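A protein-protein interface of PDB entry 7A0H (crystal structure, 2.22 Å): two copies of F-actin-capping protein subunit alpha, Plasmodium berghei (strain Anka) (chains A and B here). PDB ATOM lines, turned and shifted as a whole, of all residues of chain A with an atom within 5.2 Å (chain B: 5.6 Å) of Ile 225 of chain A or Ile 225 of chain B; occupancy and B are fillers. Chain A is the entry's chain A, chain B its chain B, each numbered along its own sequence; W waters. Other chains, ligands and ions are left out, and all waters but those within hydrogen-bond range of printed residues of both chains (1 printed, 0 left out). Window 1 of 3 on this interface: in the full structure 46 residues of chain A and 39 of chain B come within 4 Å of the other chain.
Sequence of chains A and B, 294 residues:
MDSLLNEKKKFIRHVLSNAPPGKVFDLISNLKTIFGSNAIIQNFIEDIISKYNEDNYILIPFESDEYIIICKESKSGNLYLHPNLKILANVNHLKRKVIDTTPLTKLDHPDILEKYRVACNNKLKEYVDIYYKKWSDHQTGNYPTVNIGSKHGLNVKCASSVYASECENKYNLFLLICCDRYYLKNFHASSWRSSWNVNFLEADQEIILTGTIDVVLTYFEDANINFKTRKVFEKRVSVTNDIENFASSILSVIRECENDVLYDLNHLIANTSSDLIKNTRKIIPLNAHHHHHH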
ATOM      1  N   PRO A  20      16.341  15.591 -19.594  1.00  0.00           N
ATOM      2  CA  PRO A  20      17.675  16.243 -19.720  1.00  0.00           C
ATOM      3  C   PRO A  20      18.337  15.875 -21.038  1.00  0.00           C
ATOM      4  O   PRO A  20      18.005  14.839 -21.635  1.00  0.00           O
ATOM      5  CB  PRO A  20      18.458  15.700 -18.514  1.00  0.00           C
ATOM      6  CG  PRO A  20      17.809  14.347 -18.237  1.00  0.00           C
ATOM      7  CD  PRO A  20      16.358  14.523 -18.573  1.00  0.00           C
ATOM      8  N   PRO A  21      19.265  16.695 -21.539  1.00  0.00           N
ATOM      9  CA  PRO A  21      19.757  16.463 -22.901  1.00  0.00           C
ATOM     10  C   PRO A  21      20.228  15.041 -23.092  1.00  0.00           C
ATOM     11  O   PRO A  21      19.939  14.413 -24.107  1.00  0.00           O
ATOM     12  CB  PRO A  21      20.923  17.449 -23.038  1.00  0.00           C
ATOM     13  CG  PRO A  21      20.706  18.493 -22.018  1.00  0.00           C
ATOM     14  CD  PRO A  21      19.946  17.833 -20.888  1.00  0.00           C
ATOM     15  N   LEU A 217      25.659  22.361 -17.123  1.00  0.00           N
ATOM     16  CA  LEU A 217      26.259  21.107 -16.685  1.00  0.00           C
ATOM     17  C   LEU A 217      25.179  20.039 -16.945  1.00  0.00           C
ATOM     18  O   LEU A 217      23.996  20.210 -16.575  1.00  0.00           O
ATOM     19  CB  LEU A 217      26.646  21.154 -15.213  1.00  0.00           C
ATOM     20  CG  LEU A 217      27.389  19.947 -14.599  1.00  0.00           C
ATOM     21  CD1 LEU A 217      28.867  19.810 -15.260  1.00  0.00           C
ATOM     22  CD2 LEU A 217      27.446  20.021 -13.101  1.00  0.00           C
ATOM     23  N   THR A 218      25.592  18.956 -17.607  1.00  0.00           N
ATOM     24  CA  THR A 218      24.694  17.889 -18.024  1.00  0.00           C
ATOM     25  C   THR A 218      25.136  16.498 -17.590  1.00  0.00           C
ATOM     26  O   THR A 218      24.343  15.566 -17.725  1.00  0.00           O
ATOM     27  CB  THR A 218      24.477  17.891 -19.568  1.00  0.00           C
ATOM     28  OG1 THR A 218      25.694  17.659 -20.316  1.00  0.00           O
ATOM     29  CG2 THR A 218      23.789  19.175 -20.015  1.00  0.00           C
ATOM     30  N   TYR A 219      26.345  16.336 -17.047  1.00  0.00           N
ATOM     31  CA  TYR A 219      26.777  15.097 -16.437  1.00  0.00           C
ATOM     32  C   TYR A 219      27.257  15.445 -15.040  1.00  0.00           C
ATOM     33  O   TYR A 219      28.095  16.345 -14.873  1.00  0.00           O
ATOM     34  CB  TYR A 219      27.859  14.397 -17.231  1.00  0.00           C
ATOM     35  CG  TYR A 219      27.787  12.888 -17.072  1.00  0.00           C
ATOM     36  CD1 TYR A 219      26.767  12.161 -17.671  1.00  0.00           C
ATOM     37  CD2 TYR A 219      28.737  12.194 -16.331  1.00  0.00           C
ATOM     38  CE1 TYR A 219      26.685  10.782 -17.531  1.00  0.00           C
ATOM     39  CE2 TYR A 219      28.671  10.810 -16.192  1.00  0.00           C
ATOM     40  CZ  TYR A 219      27.633  10.114 -16.790  1.00  0.00           C
ATOM     41  OH  TYR A 219      27.538   8.747 -16.669  1.00  0.00           O
ATOM     42  N   PHE A 220      26.763  14.701 -14.045  1.00  0.00           N
ATOM     43  CA  PHE A 220      27.078  14.993 -12.651  1.00  0.00           C
ATOM     44  C   PHE A 220      26.800  13.742 -11.830  1.00  0.00           C
ATOM     45  O   PHE A 220      25.637  13.327 -11.668  1.00  0.00           O
ATOM     46  CB  PHE A 220      26.274  16.203 -12.153  1.00  0.00           C
ATOM     47  CG  PHE A 220      26.515  16.546 -10.678  1.00  0.00           C
ATOM     48  CD1 PHE A 220      27.745  17.008 -10.254  1.00  0.00           C
ATOM     49  CD2 PHE A 220      25.509  16.400  -9.723  1.00  0.00           C
ATOM     50  CE1 PHE A 220      27.981  17.312  -8.906  1.00  0.00           C
ATOM     51  CE2 PHE A 220      25.729  16.709  -8.377  1.00  0.00           C
ATOM     52  CZ  PHE A 220      26.980  17.179  -7.964  1.00  0.00           C
ATOM     53  N   ALA A 223      24.964  10.954 -13.548  1.00  0.00           N
ATOM     54  CA  ALA A 223      23.608  11.189 -13.996  1.00  0.00           C
ATOM     55  C   ALA A 223      23.580  12.234 -15.102  1.00  0.00           C
ATOM     56  O   ALA A 223      24.362  13.200 -15.104  1.00  0.00           O
ATOM     57  CB  ALA A 223      22.672  11.662 -12.886  1.00  0.00           C
ATOM     58  N   ASN A 224      22.630  12.073 -15.992  1.00  0.00           N
ATOM     59  CA  ASN A 224      22.310  13.120 -16.942  1.00  0.00           C
ATOM     60  C   ASN A 224      21.515  14.183 -16.204  1.00  0.00           C
ATOM     61  O   ASN A 224      20.463  13.885 -15.640  1.00  0.00           O
ATOM     62  CB  ASN A 224      21.504  12.588 -18.125  1.00  0.00           C
ATOM     63  CG  ASN A 224      22.288  11.605 -18.962  1.00  0.00           C
ATOM     64  OD1 ASN A 224      23.217  11.985 -19.664  1.00  0.00           O
ATOM     65  ND2 ASN A 224      21.904  10.352 -18.910  1.00  0.00           N
ATOM     66  N   ILE A 225      22.051  15.392 -16.116  1.00  0.00           N
ATOM     67  CA  ILE A 225      21.256  16.483 -15.577  1.00  0.00           C
ATOM     68  C   ILE A 225      21.171  17.640 -16.572  1.00  0.00           C
ATOM     69  O   ILE A 225      21.480  17.489 -17.759  1.00  0.00           O
ATOM     70  CB  ILE A 225      21.834  16.946 -14.231  1.00  0.00           C
ATOM     71  CG1 ILE A 225      23.233  17.575 -14.415  1.00  0.00           C
ATOM     72  CG2 ILE A 225      21.868  15.781 -13.254  1.00  0.00           C
ATOM     73  CD1 ILE A 225      23.706  18.374 -13.152  1.00  0.00           C
ATOM     74  N   ASN A 226      20.789  18.825 -16.082  1.00  0.00           N
ATOM     75  CA  ASN A 226      20.524  19.957 -16.971  1.00  0.00           C
ATOM     76  C   ASN A 226      20.567  21.218 -16.127  1.00  0.00           C
ATOM     77  O   ASN A 226      19.564  21.930 -16.012  1.00  0.00           O
ATOM     78  CB  ASN A 226      19.186  19.761 -17.672  1.00  0.00           C
ATOM     79  CG  ASN A 226      18.968  20.679 -18.856  1.00  0.00           C
ATOM     80  OD1 ASN A 226      19.896  21.276 -19.477  1.00  0.00           O
ATOM     81  ND2 ASN A 226      17.699  20.769 -19.223  1.00  0.00           N
ATOM     82  N   PHE A 227      21.730  21.471 -15.527  1.00  0.00           N
ATOM     83  CA  PHE A 227      21.921  22.583 -14.610  1.00  0.00           C
ATOM     84  C   PHE A 227      22.444  23.803 -15.389  1.00  0.00           C
ATOM     85  O   PHE A 227      23.584  23.838 -15.860  1.00  0.00           O
ATOM     86  CB  PHE A 227      22.897  22.158 -13.521  1.00  0.00           C
ATOM     87  CG  PHE A 227      23.279  23.272 -12.600  1.00  0.00           C
ATOM     88  CD1 PHE A 227      24.590  23.648 -12.463  1.00  0.00           C
ATOM     89  CD2 PHE A 227      22.317  23.908 -11.843  1.00  0.00           C
ATOM     90  CE1 PHE A 227      24.940  24.666 -11.626  1.00  0.00           C
ATOM     91  CE2 PHE A 227      22.648  24.885 -10.965  1.00  0.00           C
ATOM     92  CZ  PHE A 227      23.967  25.293 -10.879  1.00  0.00           C
ATOM     93  N   LEU B 217      14.948  14.481  -1.967  1.00  0.00           N
ATOM     94  CA  LEU B 217      15.093  15.905  -2.195  1.00  0.00           C
ATOM     95  C   LEU B 217      15.444  16.168  -3.643  1.00  0.00           C
ATOM     96  O   LEU B 217      16.162  15.384  -4.268  1.00  0.00           O
ATOM     97  CB  LEU B 217      16.103  16.460  -1.187  1.00  0.00           C
ATOM     98  CG  LEU B 217      16.656  17.892  -1.348  1.00  0.00           C
ATOM     99  CD1 LEU B 217      15.789  19.273  -1.474  1.00  0.00           C
ATOM    100  CD2 LEU B 217      17.619  17.875  -0.064  1.00  0.00           C
ATOM    101  N   THR B 218      14.821  17.209  -4.204  1.00  0.00           N
ATOM    102  CA  THR B 218      15.137  17.660  -5.550  1.00  0.00           C
ATOM    103  C   THR B 218      15.475  19.152  -5.509  1.00  0.00           C
ATOM    104  O   THR B 218      14.763  19.966  -4.898  1.00  0.00           O
ATOM    105  CB  THR B 218      14.007  17.430  -6.550  1.00  0.00           C
ATOM    106  OG1 THR B 218      12.897  18.260  -6.201  1.00  0.00           O
ATOM    107  CG2 THR B 218      13.562  15.928  -6.557  1.00  0.00           C
ATOM    108  N   TYR B 219      16.533  19.497  -6.215  1.00  0.00           N
ATOM    109  CA  TYR B 219      16.933  20.878  -6.324  1.00  0.00           C
ATOM    110  C   TYR B 219      15.959  21.683  -7.165  1.00  0.00           C
ATOM    111  O   TYR B 219      15.463  21.232  -8.203  1.00  0.00           O
ATOM    112  CB  TYR B 219      18.331  20.961  -6.922  1.00  0.00           C
ATOM    113  CG  TYR B 219      19.466  20.691  -5.983  1.00  0.00           C
ATOM    114  CD1 TYR B 219      19.518  19.551  -5.229  1.00  0.00           C
ATOM    115  CD2 TYR B 219      20.514  21.587  -5.865  1.00  0.00           C
ATOM    116  CE1 TYR B 219      20.583  19.311  -4.384  1.00  0.00           C
ATOM    117  CE2 TYR B 219      21.556  21.349  -5.037  1.00  0.00           C
ATOM    118  CZ  TYR B 219      21.598  20.211  -4.298  1.00  0.00           C
ATOM    119  OH  TYR B 219      22.665  19.989  -3.475  1.00  0.00           O
ATOM    120  N   ASP B 222      17.427  22.587 -10.549  1.00  0.00           N
ATOM    121  CA  ASP B 222      17.416  21.565 -11.597  1.00  0.00           C
ATOM    122  C   ASP B 222      16.708  20.323 -11.058  1.00  0.00           C
ATOM    123  O   ASP B 222      17.243  19.645 -10.190  1.00  0.00           O
ATOM    124  CB  ASP B 222      18.855  21.201 -12.044  1.00  0.00           C
ATOM    125  CG  ASP B 222      18.900  20.103 -13.125  1.00  0.00           C
ATOM    126  OD1 ASP B 222      17.848  19.827 -13.722  1.00  0.00           O
ATOM    127  OD2 ASP B 222      19.957  19.461 -13.372  1.00  0.00           O
ATOM    128  N   ALA B 223      15.593  19.958 -11.642  1.00  0.00           N
ATOM    129  CA  ALA B 223      14.875  18.847 -11.064  1.00  0.00           C
ATOM    130  C   ALA B 223      15.517  17.520 -11.397  1.00  0.00           C
ATOM    131  O   ALA B 223      15.181  16.539 -10.748  1.00  0.00           O
ATOM    132  CB  ALA B 223      13.434  18.850 -11.538  1.00  0.00           C
ATOM    133  N   ASN B 224      16.501  17.486 -12.312  1.00  0.00           N
ATOM    134  CA  ASN B 224      17.247  16.257 -12.558  1.00  0.00           C
ATOM    135  C   ASN B 224      18.281  15.998 -11.475  1.00  0.00           C
ATOM    136  O   ASN B 224      18.860  14.909 -11.437  1.00  0.00           O
ATOM    137  CB  ASN B 224      17.936  16.286 -13.925  1.00  0.00           C
ATOM    138  CG  ASN B 224      16.965  16.491 -15.065  1.00  0.00           C
ATOM    139  OD1 ASN B 224      16.211  15.597 -15.433  1.00  0.00           O
ATOM    140  ND2 ASN B 224      16.963  17.700 -15.614  1.00  0.00           N
ATOM    141  N   ILE B 225      18.449  16.930 -10.536  1.00  0.00           N
ATOM    142  CA  ILE B 225      19.339  16.769  -9.398  1.00  0.00           C
ATOM    143  C   ILE B 225      18.468  16.435  -8.204  1.00  0.00           C
ATOM    144  O   ILE B 225      17.800  17.312  -7.631  1.00  0.00           O
ATOM    145  CB  ILE B 225      20.131  18.039  -9.103  1.00  0.00           C
ATOM    146  CG1 ILE B 225      21.167  18.299 -10.161  1.00  0.00           C
ATOM    147  CG2 ILE B 225      20.807  17.923  -7.767  1.00  0.00           C
ATOM    148  CD1 ILE B 225      21.551  19.708 -10.175  1.00  0.00           C
ATOM    149  N   ASN B 226      18.525  15.173  -7.808  1.00  0.00           N
ATOM    150  CA  ASN B 226      17.641  14.640  -6.789  1.00  0.00           C
ATOM    151  C   ASN B 226      18.263  13.372  -6.250  1.00  0.00           C
ATOM    152  O   ASN B 226      19.009  12.691  -6.954  1.00  0.00           O
ATOM    153  CB  ASN B 226      16.264  14.312  -7.339  1.00  0.00           C
ATOM    154  CG  ASN B 226      16.330  13.328  -8.468  1.00  0.00           C
ATOM    155  OD1 ASN B 226      16.827  12.206  -8.311  1.00  0.00           O
ATOM    156  ND2 ASN B 226      15.849  13.744  -9.631  1.00  0.00           N
ATOM    157  N   PHE B 227      17.938  13.065  -5.003  1.00  0.00           N
ATOM    158  CA  PHE B 227      18.494  11.878  -4.356  1.00  0.00           C
ATOM    159  C   PHE B 227      17.666  11.513  -3.131  1.00  0.00           C
ATOM    160  O   PHE B 227      16.863  12.313  -2.632  1.00  0.00           O
ATOM    161  CB  PHE B 227      19.973  12.083  -3.985  1.00  0.00           C
ATOM    162  CG  PHE B 227      20.241  13.335  -3.203  1.00  0.00           C
ATOM    163  CD1 PHE B 227      21.000  14.359  -3.753  1.00  0.00           C
ATOM    164  CD2 PHE B 227      19.739  13.489  -1.923  1.00  0.00           C
ATOM    165  CE1 PHE B 227      21.256  15.514  -3.030  1.00  0.00           C
ATOM    166  CE2 PHE B 227      19.986  14.643  -1.205  1.00  0.00           C
ATOM    167  CZ  PHE B 227      20.745  15.659  -1.762  1.00  0.00           C
ATOM    168  N   THR B 272      26.870  18.483  -1.922  1.00  0.00           N
ATOM    169  CA  THR B 272      26.503  18.257  -3.308  1.00  0.00           C
ATOM    170  C   THR B 272      26.522  19.558  -4.071  1.00  0.00           C
ATOM    171  O   THR B 272      27.106  19.638  -5.157  1.00  0.00           O
ATOM    172  CB  THR B 272      25.121  17.613  -3.365  1.00  0.00           C
ATOM    173  OG1 THR B 272      25.118  16.455  -2.522  1.00  0.00           O
ATOM    174  CG2 THR B 272      24.753  17.206  -4.763  1.00  0.00           C
ATOM    175  N   LEU B 276      28.586  20.567  -7.380  1.00  0.00           N
ATOM    176  CA  LEU B 276      27.918  21.137  -8.534  1.00  0.00           C
ATOM    177  C   LEU B 276      28.679  22.379  -8.994  1.00  0.00           C
ATOM    178  O   LEU B 276      29.031  22.509 -10.167  1.00  0.00           O
ATOM    179  CB  LEU B 276      26.494  21.433  -8.099  1.00  0.00           C
ATOM    180  CG  LEU B 276      25.310  21.459  -9.039  1.00  0.00           C
ATOM    181  CD1 LEU B 276      25.330  20.351 -10.038  1.00  0.00           C
ATOM    182  CD2 LEU B 276      24.121  21.290  -8.082  1.00  0.00           C
HETATM  183  O   HOH W   1      15.245  18.744 -18.214  1.00  0.00           O
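Water W1 lies within hydrogen-bond range of the side-chain amide nitrogen of Asn 224 of chain B (3.3 Å) and the side-chain amide nitrogen of Asn 226 of chain A (3.3 Å).
Asn 224 of chain A touches its own counterpart, Asn 224 of chain B. Ile 225 of chain A touches Asn 224 of chain B, but with the chains exchanged Asn 224 of chain A does not touch Ile 225 of chain B (6.3 Å). Ile 225 of chain A touches its own counterpart, Ile 225 of chain B. Asn 226 of chain A touches Asn 224 of chain B, but with the chains exchanged Asn 224 of chain A does not touch Asn 226 of chain B (7.6 Å). Of the 11 pairs that touch across the chains among the printed residues, 2 have their exchanged pair printed and touching as well.
The backbone NH (N) of Tyr 219 of chain B is in hydrogen-bond range of the backbone carbonyl oxygen (O) of Ile 225 of chain B, at 2.9 Å. The side-chain amide nitrogen (ND2) of Asn 224 of chain B lies within hydrogen-bond range of the side-chain carboxylate (OD1) of Asp 222 of chain B (3.0 Å). The backbone carbonyl oxygen (O) of Thr 218 of chain A lies within hydrogen-bond range of the backbone NH (N) of Ile 225 of chain A, 2.8 Å away. The backbone NH (N) of Phe 227 of chain A sits at hydrogen-bond distance from the backbone carbonyl oxygen (O) of Leu 217 of chain A (2.8 Å).
Pro 20 of chain A touches Asn 224 of chain B (CD to OD1, 3.3 Å). CD2 of Leu 217 of chain A touches CD1 of Leu 276 of chain B, 3.7 Å away. Phe 220 of chain A touches Thr 272 of chain B (CZ to O, 3.7 Å). CE1 of Phe 220 of chain A touches N of Leu 276 of chain B, 3.6 Å away. Asn 224 of chain A touches Asn 224 of chain B (O to CB, 3.9 Å). Asp 222 of chain B touches Ile 225 of chain A (OD2 to CB, 3.3 Å). O of Asn 224 of chain B touches CG2 of Ile 225 of chain A (3.6 Å). Ile 225 of chain B touches Ile 225 of chain A (CD1 to CD1, 3.9 Å). Asn 224 of chain B touches Asn 226 of chain A (ND2 to CB, 3.7 Å).
Of chain B, only Asp 222 (3.3 Å), Asn 224 (3.6 Å) and Ile 225 (3.9 Å) come within 4 Å of Ile 225 of chain A. Of the printed residues of chain B, Phe 227 of chain A touches Asp 222. Of the printed residues of chain A, Asn 224 of chain B touches Pro 20, Asn 224, Ile 225 and Asn 226. Ala 223 of chain A touches none of the printed residues of chain B. Tyr 219 of chain A touches none of the printed residues of chain B. The nearest residue of chain B that does not touch Ile 225 of chain A is Leu 276 of chain B (4.03 Å).
The backbone NH of Phe 227 of chain A lies within hydrogen-bond range of the side-chain carboxylate of Asp 222 of chain B (3.4 Å). The backbone NH (N) of Asn 226 of chain A lies within hydrogen-bond range of the side-chain carboxylate (OD2) of Asp 222 of chain B (2.9 Å).
Of the 11 printed residues of chain B, 5 touch a printed residue of chain A. Of the 11 printed residues of chain A, 7 touch a printed residue of chain B. Hydrophobic or aromatic side chains of chain A within 4 Å of the printed part of chain B: Pro 20, Leu 217, Phe 220, Ile 225 and Phe 227. Among the printed residues, 11 pairs touch across the chains. Among the printed residues, no Asp or Glu carboxylate lies within 4 Å of a Lys or Arg side-chain nitrogen of the other chain.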
